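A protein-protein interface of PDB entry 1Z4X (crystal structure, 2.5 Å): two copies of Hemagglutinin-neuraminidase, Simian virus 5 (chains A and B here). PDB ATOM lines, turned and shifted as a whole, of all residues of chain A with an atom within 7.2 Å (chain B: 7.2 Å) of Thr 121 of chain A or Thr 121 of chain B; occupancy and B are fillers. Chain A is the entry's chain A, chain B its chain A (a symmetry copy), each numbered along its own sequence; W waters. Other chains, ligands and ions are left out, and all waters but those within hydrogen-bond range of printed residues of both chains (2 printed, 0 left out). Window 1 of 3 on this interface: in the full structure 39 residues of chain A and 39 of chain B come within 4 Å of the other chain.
The backbone NH (N) of Thr 123 of chain B is in hydrogen-bond range of the side-chain amide oxygen (OD1) of Asn 114 of chain A (2.8 Å).
The backbone NH of Ser 117 of chain A is in hydrogen-bond range of the backbone carbonyl oxygen of Thr 121 of chain B (2.8 Å).
The backbone NH (N) of Met 115 of chain A sits at hydrogen-bond distance from the side-chain hydroxyl (OG1) of Thr 123 of chain B, 3.0 Å away.
The backbone carbonyl oxygen (O) of Thr 121 of chain A is in hydrogen-bond range of the backbone NH (N) of Ser 117 of chain B (2.8 Å).
The side-chain hydroxyl (OG1) of Thr 123 of chain A sits at hydrogen-bond distance from the backbone NH (N) of Met 115 of chain B.
OD1 of Asn 114 of chain B lies within hydrogen-bond range of N of Thr 123 of chain A, at 2.8 Å.
OG of Ser 117 of chain B lies within hydrogen-bond range of N of Ile 119 of chain B (3.2 Å).
N of Ile 119 of chain A sits at hydrogen-bond distance from OG of Ser 117 of chain A (3.2 Å).
The backbone carbonyl oxygen of Thr 124 of chain B lies within hydrogen-bond range of the backbone NH of Gly 518 of chain B (2.7 Å).
Ser 117 of chain B touches Pro 120 of chain A.
Thr 121 of chain A touches Pro 116 of chain B.
OG1 of Thr 121 of chain A touches OG1 of Thr 121 of chain B, at 3.7 Å.
NE2 of Gln 521 of chain B touches CG2 of Thr 121 of chain A, 3.3 Å away.
Asn 114 of chain B touches Ala 122 of chain A.
Thr 121 of chain B touches just these residues of chain A: Met 115 (3.6 Å), Pro 116 (3.7 Å), Ser 117 (2.8 Å), Thr 121 (3.7 Å) and Gln 521 (3.3 Å).
Of the printed residues of chain B, Met 115 of chain A touches Thr 121 and Thr 123.
Printed residues of chain B within 4 Å of Ala 122 of chain A: Asn 114 (3.2 Å).
Of the printed residues of chain B, Gln 521 of chain A touches Thr 121 and Gln 521.
Thr 129 of chain B touches none of the printed residues of chain A.
The nearest residue of chain B that does not touch Thr 121 of chain A is Asn 114 of chain B (5.2 Å).
The nearest printed residue of chain B that does not touch Asn 114 of chain A is Thr 121 of chain B (5.2 Å).
Of the 20 printed residues of chain B, 11 touch a printed residue of chain A.
Printed residues of chain B that touch a printed residue of chain A: Asn 114, Met 115, Pro 116, Ser 117, Pro 120, Thr 121, Ala 122, Thr 123, Thr 124, Gln 521 and Pro 524.
Hydrophobic or aromatic side chains of chain A within 4 Å of the printed part of chain B: Met 115, Pro 120, Ala 122 and Pro 524.
Among the printed residues, 22 pairs touch across the chains.
Among the printed residues, no Asp or Glu carboxylate lies within 4 Å of a Lys or Arg side-chain nitrogen of the other chain.
Ser 117 of chain A touches Pro 120 of chain B, and with the chains exchanged Pro 120 of chain A touches Ser 117 of chain B.
Thr 121 of chain B touches its own counterpart, Thr 121 of chain A.
Of the 22 pairs that touch across the chains among the printed residues, 22 have their exchanged pair printed and touching as well.
Water W2 lies within hydrogen-bond range of O of Ile 119 of chain B (2.7 Å), N of Thr 121 of chain A (2.9 Å) and OG of Ser 117 of chain B (3.4 Å).
Water W1 lies within hydrogen-bond range of O of Ile 119 of chain A (2.7 Å), N of Thr 121 of chain B (2.9 Å) and OG of Ser 117 of chain A (3.4 Å).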
ATOM      1  N   ASN A 114      15.804 -25.500  15.557  1.00  0.00           N
ATOM      2  CA  ASN A 114      15.382 -24.342  16.328  1.00  0.00           C
ATOM      3  C   ASN A 114      14.194 -23.587  15.769  1.00  0.00           C
ATOM      4  O   ASN A 114      14.262 -23.012  14.686  1.00  0.00           O
ATOM      5  CB  ASN A 114      16.532 -23.352  16.504  1.00  0.00           C
ATOM      6  CG  ASN A 114      16.143 -22.177  17.385  1.00  0.00           C
ATOM      7  OD1 ASN A 114      15.892 -22.339  18.576  1.00  0.00           O
ATOM      8  ND2 ASN A 114      16.078 -20.993  16.799  1.00  0.00           N
ATOM      9  N   MET A 115      13.106 -23.576  16.531  1.00  0.00           N
ATOM     10  CA  MET A 115      11.902 -22.863  16.148  1.00  0.00           C
ATOM     11  C   MET A 115      11.455 -22.058  17.360  1.00  0.00           C
ATOM     12  O   MET A 115      11.839 -22.363  18.484  1.00  0.00           O
ATOM     13  CB  MET A 115      10.793 -23.839  15.743  1.00  0.00           C
ATOM     14  CG  MET A 115      10.297 -24.713  16.874  1.00  0.00           C
ATOM     15  SD  MET A 115       8.861 -25.711  16.445  1.00  0.00           S
ATOM     16  CE  MET A 115       8.450 -26.399  18.052  1.00  0.00           C
ATOM     17  N   PRO A 116      10.655 -21.003  17.152  1.00  0.00           N
ATOM     18  CA  PRO A 116      10.204 -20.215  18.303  1.00  0.00           C
ATOM     19  C   PRO A 116       9.252 -21.071  19.134  1.00  0.00           C
ATOM     20  O   PRO A 116       8.247 -21.569  18.625  1.00  0.00           O
ATOM     21  CB  PRO A 116       9.493 -19.029  17.653  1.00  0.00           C
ATOM     22  CG  PRO A 116      10.178 -18.906  16.316  1.00  0.00           C
ATOM     23  CD  PRO A 116      10.290 -20.343  15.889  1.00  0.00           C
ATOM     24  N   SER A 117       9.568 -21.254  20.407  1.00  0.00           N
ATOM     25  CA  SER A 117       8.731 -22.060  21.280  1.00  0.00           C
ATOM     26  C   SER A 117       7.350 -21.457  21.470  1.00  0.00           C
ATOM     27  O   SER A 117       7.215 -20.254  21.677  1.00  0.00           O
ATOM     28  CB  SER A 117       9.401 -22.238  22.642  1.00  0.00           C
ATOM     29  OG  SER A 117       8.579 -22.999  23.516  1.00  0.00           O
ATOM     30  N   PHE A 118       6.323 -22.301  21.391  1.00  0.00           N
ATOM     31  CA  PHE A 118       4.948 -21.847  21.578  1.00  0.00           C
ATOM     32  C   PHE A 118       4.495 -22.103  23.020  1.00  0.00           C
ATOM     33  O   PHE A 118       3.357 -21.811  23.384  1.00  0.00           O
ATOM     34  CB  PHE A 118       4.016 -22.559  20.584  1.00  0.00           C
ATOM     35  CG  PHE A 118       3.997 -24.061  20.724  1.00  0.00           C
ATOM     36  CD1 PHE A 118       3.081 -24.687  21.557  1.00  0.00           C
ATOM     37  CD2 PHE A 118       4.906 -24.843  20.017  1.00  0.00           C
ATOM     38  CE1 PHE A 118       3.073 -26.081  21.684  1.00  0.00           C
ATOM     39  CE2 PHE A 118       4.903 -26.226  20.140  1.00  0.00           C
ATOM     40  CZ  PHE A 118       3.987 -26.849  20.973  1.00  0.00           C
ATOM     41  N   ILE A 119       5.393 -22.649  23.836  1.00  0.00           N
ATOM     42  CA  ILE A 119       5.086 -22.931  25.237  1.00  0.00           C
ATOM     43  C   ILE A 119       5.715 -21.840  26.102  1.00  0.00           C
ATOM     44  O   ILE A 119       6.934 -21.683  26.131  1.00  0.00           O
ATOM     45  CB  ILE A 119       5.623 -24.315  25.647  1.00  0.00           C
ATOM     46  CG1 ILE A 119       5.001 -25.386  24.741  1.00  0.00           C
ATOM     47  CG2 ILE A 119       5.304 -24.593  27.096  1.00  0.00           C
ATOM     48  CD1 ILE A 119       5.522 -26.782  24.977  1.00  0.00           C
ATOM     49  N   PRO A 120       4.880 -21.067  26.815  1.00  0.00           N
ATOM     50  CA  PRO A 120       5.353 -19.977  27.674  1.00  0.00           C
ATOM     51  C   PRO A 120       6.200 -20.373  28.872  1.00  0.00           C
ATOM     52  O   PRO A 120       5.943 -21.363  29.551  1.00  0.00           O
ATOM     53  CB  PRO A 120       4.063 -19.274  28.078  1.00  0.00           C
ATOM     54  CG  PRO A 120       3.102 -20.410  28.178  1.00  0.00           C
ATOM     55  CD  PRO A 120       3.416 -21.212  26.922  1.00  0.00           C
ATOM     56  N   THR A 121       7.202 -19.547  29.124  1.00  0.00           N
ATOM     57  CA  THR A 121       8.158 -19.714  30.209  1.00  0.00           C
ATOM     58  C   THR A 121       7.733 -18.946  31.474  1.00  0.00           C
ATOM     59  O   THR A 121       6.918 -18.028  31.408  1.00  0.00           O
ATOM     60  CB  THR A 121       9.539 -19.220  29.706  1.00  0.00           C
ATOM     61  OG1 THR A 121      10.207 -20.302  29.053  1.00  0.00           O
ATOM     62  CG2 THR A 121      10.386 -18.685  30.824  1.00  0.00           C
ATOM     63  N   ALA A 122       8.280 -19.334  32.622  1.00  0.00           N
ATOM     64  CA  ALA A 122       7.976 -18.658  33.881  1.00  0.00           C
ATOM     65  C   ALA A 122       8.853 -17.402  33.931  1.00  0.00           C
ATOM     66  O   ALA A 122       9.862 -17.332  33.234  1.00  0.00           O
ATOM     67  CB  ALA A 122       8.293 -19.573  35.056  1.00  0.00           C
ATOM     68  N   THR A 123       8.470 -16.411  34.732  1.00  0.00           N
ATOM     69  CA  THR A 123       9.259 -15.180  34.822  1.00  0.00           C
ATOM     70  C   THR A 123       9.875 -14.933  36.197  1.00  0.00           C
ATOM     71  O   THR A 123      10.331 -13.828  36.490  1.00  0.00           O
ATOM     72  CB  THR A 123       8.430 -13.934  34.411  1.00  0.00           C
ATOM     73  OG1 THR A 123       7.228 -13.859  35.190  1.00  0.00           O
ATOM     74  CG2 THR A 123       8.079 -14.005  32.935  1.00  0.00           C
ATOM     75  N   THR A 124       9.864 -15.955  37.045  1.00  0.00           N
ATOM     76  CA  THR A 124      10.470 -15.868  38.367  1.00  0.00           C
ATOM     77  C   THR A 124      11.232 -17.167  38.565  1.00  0.00           C
ATOM     78  O   THR A 124      10.921 -18.177  37.936  1.00  0.00           O
ATOM     79  CB  THR A 124       9.437 -15.750  39.516  1.00  0.00           C
ATOM     80  OG1 THR A 124       8.605 -16.909  39.529  1.00  0.00           O
ATOM     81  CG2 THR A 124       8.581 -14.512  39.357  1.00  0.00           C
ATOM     82  N   THR A 129       5.780 -24.269  36.089  1.00  0.00           N
ATOM     83  CA  THR A 129       4.927 -24.619  34.957  1.00  0.00           C
ATOM     84  C   THR A 129       5.064 -26.127  34.759  1.00  0.00           C
ATOM     85  O   THR A 129       6.161 -26.623  34.508  1.00  0.00           O
ATOM     86  CB  THR A 129       5.356 -23.899  33.655  1.00  0.00           C
ATOM     87  OG1 THR A 129       6.699 -24.269  33.314  1.00  0.00           O
ATOM     88  CG2 THR A 129       5.273 -22.390  33.829  1.00  0.00           C
ATOM     89  N   HIS A 145      -1.028 -26.080  30.023  1.00  0.00           N
ATOM     90  CA  HIS A 145      -0.216 -26.528  31.147  1.00  0.00           C
ATOM     91  C   HIS A 145      -0.587 -25.757  32.405  1.00  0.00           C
ATOM     92  O   HIS A 145      -1.194 -24.688  32.344  1.00  0.00           O
ATOM     93  CB  HIS A 145       1.299 -26.456  30.838  1.00  0.00           C
ATOM     94  CG  HIS A 145       1.888 -25.081  30.824  1.00  0.00           C
ATOM     95  ND1 HIS A 145       2.927 -24.733  29.990  1.00  0.00           N
ATOM     96  CD2 HIS A 145       1.641 -23.982  31.588  1.00  0.00           C
ATOM     97  CE1 HIS A 145       3.299 -23.488  30.235  1.00  0.00           C
ATOM     98  NE2 HIS A 145       2.530 -23.015  31.203  1.00  0.00           N
ATOM     99  N   LEU A 517      15.257 -19.514  34.999  1.00  0.00           N
ATOM    100  CA  LEU A 517      13.872 -19.104  35.240  1.00  0.00           C
ATOM    101  C   LEU A 517      12.932 -20.281  35.497  1.00  0.00           C
ATOM    102  O   LEU A 517      12.886 -21.231  34.722  1.00  0.00           O
ATOM    103  CB  LEU A 517      13.342 -18.289  34.053  1.00  0.00           C
ATOM    104  CG  LEU A 517      13.683 -16.798  33.973  1.00  0.00           C
ATOM    105  CD1 LEU A 517      13.087 -16.077  35.167  1.00  0.00           C
ATOM    106  CD2 LEU A 517      15.186 -16.605  33.928  1.00  0.00           C
ATOM    107  N   GLY A 518      12.188 -20.196  36.598  1.00  0.00           N
ATOM    108  CA  GLY A 518      11.240 -21.243  36.958  1.00  0.00           C
ATOM    109  C   GLY A 518      11.817 -22.575  37.409  1.00  0.00           C
ATOM    110  O   GLY A 518      13.000 -22.857  37.219  1.00  0.00           O
ATOM    111  N   PHE A 520      10.684 -25.506  36.318  1.00  0.00           N
ATOM    112  CA  PHE A 520      10.780 -26.260  35.082  1.00  0.00           C
ATOM    113  C   PHE A 520      10.591 -25.334  33.899  1.00  0.00           C
ATOM    114  O   PHE A 520      10.009 -24.254  34.018  1.00  0.00           O
ATOM    115  CB  PHE A 520       9.693 -27.348  34.994  1.00  0.00           C
ATOM    116  CG  PHE A 520       9.855 -28.469  35.974  1.00  0.00           C
ATOM    117  CD1 PHE A 520       9.403 -28.341  37.287  1.00  0.00           C
ATOM    118  CD2 PHE A 520      10.464 -29.664  35.584  1.00  0.00           C
ATOM    119  CE1 PHE A 520       9.554 -29.385  38.202  1.00  0.00           C
ATOM    120  CE2 PHE A 520      10.620 -30.714  36.487  1.00  0.00           C
ATOM    121  CZ  PHE A 520      10.163 -30.579  37.802  1.00  0.00           C
ATOM    122  N   GLN A 521      11.112 -25.759  32.760  1.00  0.00           N
ATOM    123  CA  GLN A 521      10.933 -25.035  31.519  1.00  0.00           C
ATOM    124  C   GLN A 521      10.417 -26.132  30.607  1.00  0.00           C
ATOM    125  O   GLN A 521      11.140 -27.082  30.302  1.00  0.00           O
ATOM    126  CB  GLN A 521      12.249 -24.481  30.966  1.00  0.00           C
ATOM    127  CG  GLN A 521      12.026 -23.546  29.776  1.00  0.00           C
ATOM    128  CD  GLN A 521      13.314 -23.016  29.162  1.00  0.00           C
ATOM    129  OE1 GLN A 521      14.257 -22.671  29.872  1.00  0.00           O
ATOM    130  NE2 GLN A 521      13.348 -22.929  27.836  1.00  0.00           N
ATOM    131  N   ILE A 522       9.152 -26.040  30.223  1.00  0.00           N
ATOM    132  CA  ILE A 522       8.579 -27.036  29.329  1.00  0.00           C
ATOM    133  C   ILE A 522       9.013 -26.655  27.918  1.00  0.00           C
ATOM    134  O   ILE A 522       8.636 -25.609  27.401  1.00  0.00           O
ATOM    135  CB  ILE A 522       7.055 -27.062  29.449  1.00  0.00           C
ATOM    136  CG1 ILE A 522       6.669 -27.484  30.870  1.00  0.00           C
ATOM    137  CG2 ILE A 522       6.474 -28.026  28.424  1.00  0.00           C
ATOM    138  CD1 ILE A 522       5.195 -27.469  31.154  1.00  0.00           C
ATOM    139  N   VAL A 523       9.822 -27.513  27.309  1.00  0.00           N
ATOM    140  CA  VAL A 523      10.361 -27.256  25.988  1.00  0.00           C
ATOM    141  C   VAL A 523       9.808 -28.154  24.894  1.00  0.00           C
ATOM    142  O   VAL A 523       9.729 -29.370  25.057  1.00  0.00           O
ATOM    143  CB  VAL A 523      11.894 -27.415  26.004  1.00  0.00           C
ATOM    144  CG1 VAL A 523      12.462 -27.175  24.618  1.00  0.00           C
ATOM    145  CG2 VAL A 523      12.507 -26.457  27.018  1.00  0.00           C
ATOM    146  N   PRO A 524       9.389 -27.553  23.769  1.00  0.00           N
ATOM    147  CA  PRO A 524       8.857 -28.329  22.651  1.00  0.00           C
ATOM    148  C   PRO A 524      10.007 -28.610  21.686  1.00  0.00           C
ATOM    149  O   PRO A 524      10.191 -27.898  20.697  1.00  0.00           O
ATOM    150  CB  PRO A 524       7.808 -27.393  22.051  1.00  0.00           C
ATOM    151  CG  PRO A 524       8.437 -26.057  22.231  1.00  0.00           C
ATOM    152  CD  PRO A 524       9.022 -26.130  23.636  1.00  0.00           C
ATOM    153  N   ASN B 114       5.436 -13.838  38.855  1.00  0.00           N
ATOM    154  CA  ASN B 114       5.421 -14.862  37.823  1.00  0.00           C
ATOM    155  C   ASN B 114       4.194 -14.871  36.934  1.00  0.00           C
ATOM    156  O   ASN B 114       3.083 -15.124  37.392  1.00  0.00           O
ATOM    157  CB  ASN B 114       5.577 -16.255  38.430  1.00  0.00           C
ATOM    158  CG  ASN B 114       5.659 -17.335  37.365  1.00  0.00           C
ATOM    159  OD1 ASN B 114       6.615 -17.391  36.596  1.00  0.00           O
ATOM    160  ND2 ASN B 114       4.649 -18.187  37.306  1.00  0.00           N
ATOM    161  N   MET B 115       4.411 -14.613  35.650  1.00  0.00           N
ATOM    162  CA  MET B 115       3.341 -14.624  34.669  1.00  0.00           C
ATOM    163  C   MET B 115       3.831 -15.442  33.482  1.00  0.00           C
ATOM    164  O   MET B 115       5.030 -15.626  33.308  1.00  0.00           O
ATOM    165  CB  MET B 115       3.006 -13.202  34.208  1.00  0.00           C
ATOM    166  CG  MET B 115       4.123 -12.519  33.450  1.00  0.00           C
ATOM    167  SD  MET B 115       3.655 -10.934  32.738  1.00  0.00           S
ATOM    168  CE  MET B 115       5.118 -10.570  31.761  1.00  0.00           C
ATOM    169  N   PRO B 116       2.911 -15.966  32.660  1.00  0.00           N
ATOM    170  CA  PRO B 116       3.357 -16.752  31.506  1.00  0.00           C
ATOM    171  C   PRO B 116       4.049 -15.816  30.518  1.00  0.00           C
ATOM    172  O   PRO B 116       3.464 -14.827  30.074  1.00  0.00           O
ATOM    173  CB  PRO B 116       2.051 -17.316  30.947  1.00  0.00           C
ATOM    174  CG  PRO B 116       1.154 -17.373  32.156  1.00  0.00           C
ATOM    175  CD  PRO B 116       1.454 -16.063  32.830  1.00  0.00           C
ATOM    176  N   SER B 117       5.294 -16.116  30.182  1.00  0.00           N
ATOM    177  CA  SER B 117       6.042 -15.281  29.256  1.00  0.00           C
ATOM    178  C   SER B 117       5.425 -15.268  27.868  1.00  0.00           C
ATOM    179  O   SER B 117       5.035 -16.309  27.345  1.00  0.00           O
ATOM    180  CB  SER B 117       7.491 -15.758  29.164  1.00  0.00           C
ATOM    181  OG  SER B 117       8.227 -14.970  28.239  1.00  0.00           O
ATOM    182  N   PHE B 118       5.333 -14.078  27.275  1.00  0.00           N
ATOM    183  CA  PHE B 118       4.780 -13.936  25.933  1.00  0.00           C
ATOM    184  C   PHE B 118       5.907 -13.889  24.895  1.00  0.00           C
ATOM    185  O   PHE B 118       5.656 -13.753  23.698  1.00  0.00           O
ATOM    186  CB  PHE B 118       3.914 -12.669  25.848  1.00  0.00           C
ATOM    187  CG  PHE B 118       4.659 -11.392  26.144  1.00  0.00           C
ATOM    188  CD1 PHE B 118       5.269 -10.671  25.127  1.00  0.00           C
ATOM    189  CD2 PHE B 118       4.749 -10.918  27.449  1.00  0.00           C
ATOM    190  CE1 PHE B 118       5.961  -9.488  25.411  1.00  0.00           C
ATOM    191  CE2 PHE B 118       5.437  -9.746  27.737  1.00  0.00           C
ATOM    192  CZ  PHE B 118       6.044  -9.028  26.719  1.00  0.00           C
ATOM    193  N   ILE B 119       7.148 -14.004  25.361  1.00  0.00           N
ATOM    194  CA  ILE B 119       8.308 -13.985  24.471  1.00  0.00           C
ATOM    195  C   ILE B 119       8.793 -15.419  24.274  1.00  0.00           C
ATOM    196  O   ILE B 119       9.207 -16.081  25.225  1.00  0.00           O
ATOM    197  CB  ILE B 119       9.434 -13.114  25.059  1.00  0.00           C
ATOM    198  CG1 ILE B 119       8.909 -11.689  25.277  1.00  0.00           C
ATOM    199  CG2 ILE B 119      10.627 -13.106  24.133  1.00  0.00           C
ATOM    200  CD1 ILE B 119       9.891 -10.757  25.942  1.00  0.00           C
ATOM    201  N   PRO B 120       8.740 -15.918  23.029  1.00  0.00           N
ATOM    202  CA  PRO B 120       9.162 -17.285  22.707  1.00  0.00           C
ATOM    203  C   PRO B 120      10.636 -17.605  22.900  1.00  0.00           C
ATOM    204  O   PRO B 120      11.518 -16.809  22.596  1.00  0.00           O
ATOM    205  CB  PRO B 120       8.714 -17.451  21.260  1.00  0.00           C
ATOM    206  CG  PRO B 120       8.918 -16.082  20.707  1.00  0.00           C
ATOM    207  CD  PRO B 120       8.341 -15.198  21.805  1.00  0.00           C
ATOM    208  N   THR B 121      10.868 -18.813  23.388  1.00  0.00           N
ATOM    209  CA  THR B 121      12.191 -19.349  23.670  1.00  0.00           C
ATOM    210  C   THR B 121      12.749 -20.159  22.484  1.00  0.00           C
ATOM    211  O   THR B 121      11.999 -20.593  21.612  1.00  0.00           O
ATOM    212  CB  THR B 121      12.085 -20.236  24.937  1.00  0.00           C
ATOM    213  OG1 THR B 121      12.256 -19.413  26.093  1.00  0.00           O
ATOM    214  CG2 THR B 121      13.096 -21.346  24.933  1.00  0.00           C
ATOM    215  N   ALA B 122      14.065 -20.345  22.453  1.00  0.00           N
ATOM    216  CA  ALA B 122      14.701 -21.124  21.394  1.00  0.00           C
ATOM    217  C   ALA B 122      14.538 -22.600  21.771  1.00  0.00           C
ATOM    218  O   ALA B 122      14.313 -22.912  22.938  1.00  0.00           O
ATOM    219  CB  ALA B 122      16.177 -20.763  21.294  1.00  0.00           C
ATOM    220  N   THR B 123      14.634 -23.503  20.798  1.00  0.00           N
ATOM    221  CA  THR B 123      14.482 -24.930  21.090  1.00  0.00           C
ATOM    222  C   THR B 123      15.741 -25.757  20.840  1.00  0.00           C
ATOM    223  O   THR B 123      15.684 -26.985  20.786  1.00  0.00           O
ATOM    224  CB  THR B 123      13.304 -25.557  20.298  1.00  0.00           C
ATOM    225  OG1 THR B 123      13.463 -25.310  18.894  1.00  0.00           O
ATOM    226  CG2 THR B 123      11.985 -24.970  20.773  1.00  0.00           C
ATOM    227  N   THR B 124      16.869 -25.080  20.662  1.00  0.00           N
ATOM    228  CA  THR B 124      18.150 -25.749  20.471  1.00  0.00           C
ATOM    229  C   THR B 124      19.150 -24.993  21.329  1.00  0.00           C
ATOM    230  O   THR B 124      18.943 -23.824  21.648  1.00  0.00           O
ATOM    231  CB  THR B 124      18.659 -25.705  19.008  1.00  0.00           C
ATOM    232  OG1 THR B 124      18.850 -24.348  18.611  1.00  0.00           O
ATOM    233  CG2 THR B 124      17.682 -26.377  18.067  1.00  0.00           C
ATOM    234  N   THR B 129      18.080 -15.879  19.895  1.00  0.00           N
ATOM    235  CA  THR B 129      16.976 -14.925  19.853  1.00  0.00           C
ATOM    236  C   THR B 129      17.504 -13.621  20.451  1.00  0.00           C
ATOM    237  O   THR B 129      17.920 -13.592  21.608  1.00  0.00           O
ATOM    238  CB  THR B 129      15.758 -15.400  20.682  1.00  0.00           C
ATOM    239  OG1 THR B 129      16.138 -15.562  22.056  1.00  0.00           O
ATOM    240  CG2 THR B 129      15.230 -16.721  20.142  1.00  0.00           C
ATOM    241  N   HIS B 145      11.298  -9.871  17.812  1.00  0.00           N
ATOM    242  CA  HIS B 145      12.719 -10.113  18.027  1.00  0.00           C
ATOM    243  C   HIS B 145      13.289 -10.945  16.889  1.00  0.00           C
ATOM    244  O   HIS B 145      12.558 -11.601  16.147  1.00  0.00           O
ATOM    245  CB  HIS B 145      13.001 -10.740  19.414  1.00  0.00           C
ATOM    246  CG  HIS B 145      12.627 -12.180  19.556  1.00  0.00           C
ATOM    247  ND1 HIS B 145      12.181 -12.712  20.746  1.00  0.00           N
ATOM    248  CD2 HIS B 145      12.698 -13.226  18.687  1.00  0.00           C
ATOM    249  CE1 HIS B 145      11.994 -14.014  20.612  1.00  0.00           C
ATOM    250  NE2 HIS B 145      12.303 -14.345  19.368  1.00  0.00           N
ATOM    251  N   LEU B 517      18.715 -23.755  27.048  1.00  0.00           N
ATOM    252  CA  LEU B 517      18.220 -23.586  25.680  1.00  0.00           C
ATOM    253  C   LEU B 517      18.580 -22.230  25.075  1.00  0.00           C
ATOM    254  O   LEU B 517      18.327 -21.187  25.670  1.00  0.00           O
ATOM    255  CB  LEU B 517      16.698 -23.766  25.636  1.00  0.00           C
ATOM    256  CG  LEU B 517      16.126 -25.187  25.578  1.00  0.00           C
ATOM    257  CD1 LEU B 517      16.581 -25.864  24.300  1.00  0.00           C
ATOM    258  CD2 LEU B 517      16.571 -25.981  26.791  1.00  0.00           C
ATOM    259  N   GLY B 518      19.172 -22.267  23.883  1.00  0.00           N
ATOM    260  CA  GLY B 518      19.558 -21.047  23.186  1.00  0.00           C
ATOM    261  C   GLY B 518      20.712 -20.249  23.772  1.00  0.00           C
ATOM    262  O   GLY B 518      21.118 -20.458  24.915  1.00  0.00           O
ATOM    263  N   PHE B 520      20.631 -16.943  24.136  1.00  0.00           N
ATOM    264  CA  PHE B 520      19.969 -16.014  25.032  1.00  0.00           C
ATOM    265  C   PHE B 520      18.530 -16.438  25.239  1.00  0.00           C
ATOM    266  O   PHE B 520      17.951 -17.159  24.425  1.00  0.00           O
ATOM    267  CB  PHE B 520      19.951 -14.585  24.458  1.00  0.00           C
ATOM    268  CG  PHE B 520      21.296 -13.930  24.381  1.00  0.00           C
ATOM    269  CD1 PHE B 520      22.154 -14.183  23.312  1.00  0.00           C
ATOM    270  CD2 PHE B 520      21.710 -13.050  25.385  1.00  0.00           C
ATOM    271  CE1 PHE B 520      23.408 -13.573  23.238  1.00  0.00           C
ATOM    272  CE2 PHE B 520      22.958 -12.434  25.323  1.00  0.00           C
ATOM    273  CZ  PHE B 520      23.813 -12.692  24.247  1.00  0.00           C
ATOM    274  N   GLN B 521      17.967 -16.000  26.353  1.00  0.00           N
ATOM    275  CA  GLN B 521      16.570 -16.237  26.649  1.00  0.00           C
ATOM    276  C   GLN B 521      16.091 -14.833  26.964  1.00  0.00           C
ATOM    277  O   GLN B 521      16.512 -14.236  27.956  1.00  0.00           O
ATOM    278  CB  GLN B 521      16.372 -17.136  27.872  1.00  0.00           C
ATOM    279  CG  GLN B 521      14.910 -17.551  28.052  1.00  0.00           C
ATOM    280  CD  GLN B 521      14.662 -18.402  29.290  1.00  0.00           C
ATOM    281  OE1 GLN B 521      15.454 -19.283  29.620  1.00  0.00           O
ATOM    282  NE2 GLN B 521      13.545 -18.155  29.966  1.00  0.00           N
ATOM    283  N   ILE B 522      15.260 -14.278  26.092  1.00  0.00           N
ATOM    284  CA  ILE B 522      14.732 -12.942  26.325  1.00  0.00           C
ATOM    285  C   ILE B 522      13.570 -13.098  27.300  1.00  0.00           C
ATOM    286  O   ILE B 522      12.558 -13.716  26.984  1.00  0.00           O
ATOM    287  CB  ILE B 522      14.270 -12.303  25.015  1.00  0.00           C
ATOM    288  CG1 ILE B 522      15.476 -12.134  24.086  1.00  0.00           C
ATOM    289  CG2 ILE B 522      13.617 -10.957  25.300  1.00  0.00           C
ATOM    290  CD1 ILE B 522      15.152 -11.593  22.723  1.00  0.00           C
ATOM    291  N   VAL B 523      13.735 -12.541  28.492  1.00  0.00           N
ATOM    292  CA  VAL B 523      12.739 -12.657  29.540  1.00  0.00           C
ATOM    293  C   VAL B 523      12.011 -11.363  29.866  1.00  0.00           C
ATOM    294  O   VAL B 523      12.632 -10.315  30.028  1.00  0.00           O
ATOM    295  CB  VAL B 523      13.394 -13.173  30.836  1.00  0.00           C
ATOM    296  CG1 VAL B 523      12.363 -13.270  31.944  1.00  0.00           C
ATOM    297  CG2 VAL B 523      14.053 -14.524  30.584  1.00  0.00           C
ATOM    298  N   PRO B 524      10.672 -11.422  29.937  1.00  0.00           N
ATOM    299  CA  PRO B 524       9.881 -10.237  30.261  1.00  0.00           C
ATOM    300  C   PRO B 524       9.635 -10.235  31.769  1.00  0.00           C
ATOM    301  O   PRO B 524       8.587 -10.680  32.239  1.00  0.00           O
ATOM    302  CB  PRO B 524       8.596 -10.452  29.462  1.00  0.00           C
ATOM    303  CG  PRO B 524       8.412 -11.926  29.550  1.00  0.00           C
ATOM    304  CD  PRO B 524       9.820 -12.469  29.339  1.00  0.00           C
HETATM  305  O   HOH W   1       8.812 -19.996  25.055  1.00  0.00           O
HETATM  306  O   HOH W   2       8.308 -18.070  26.887  1.00  0.00           O
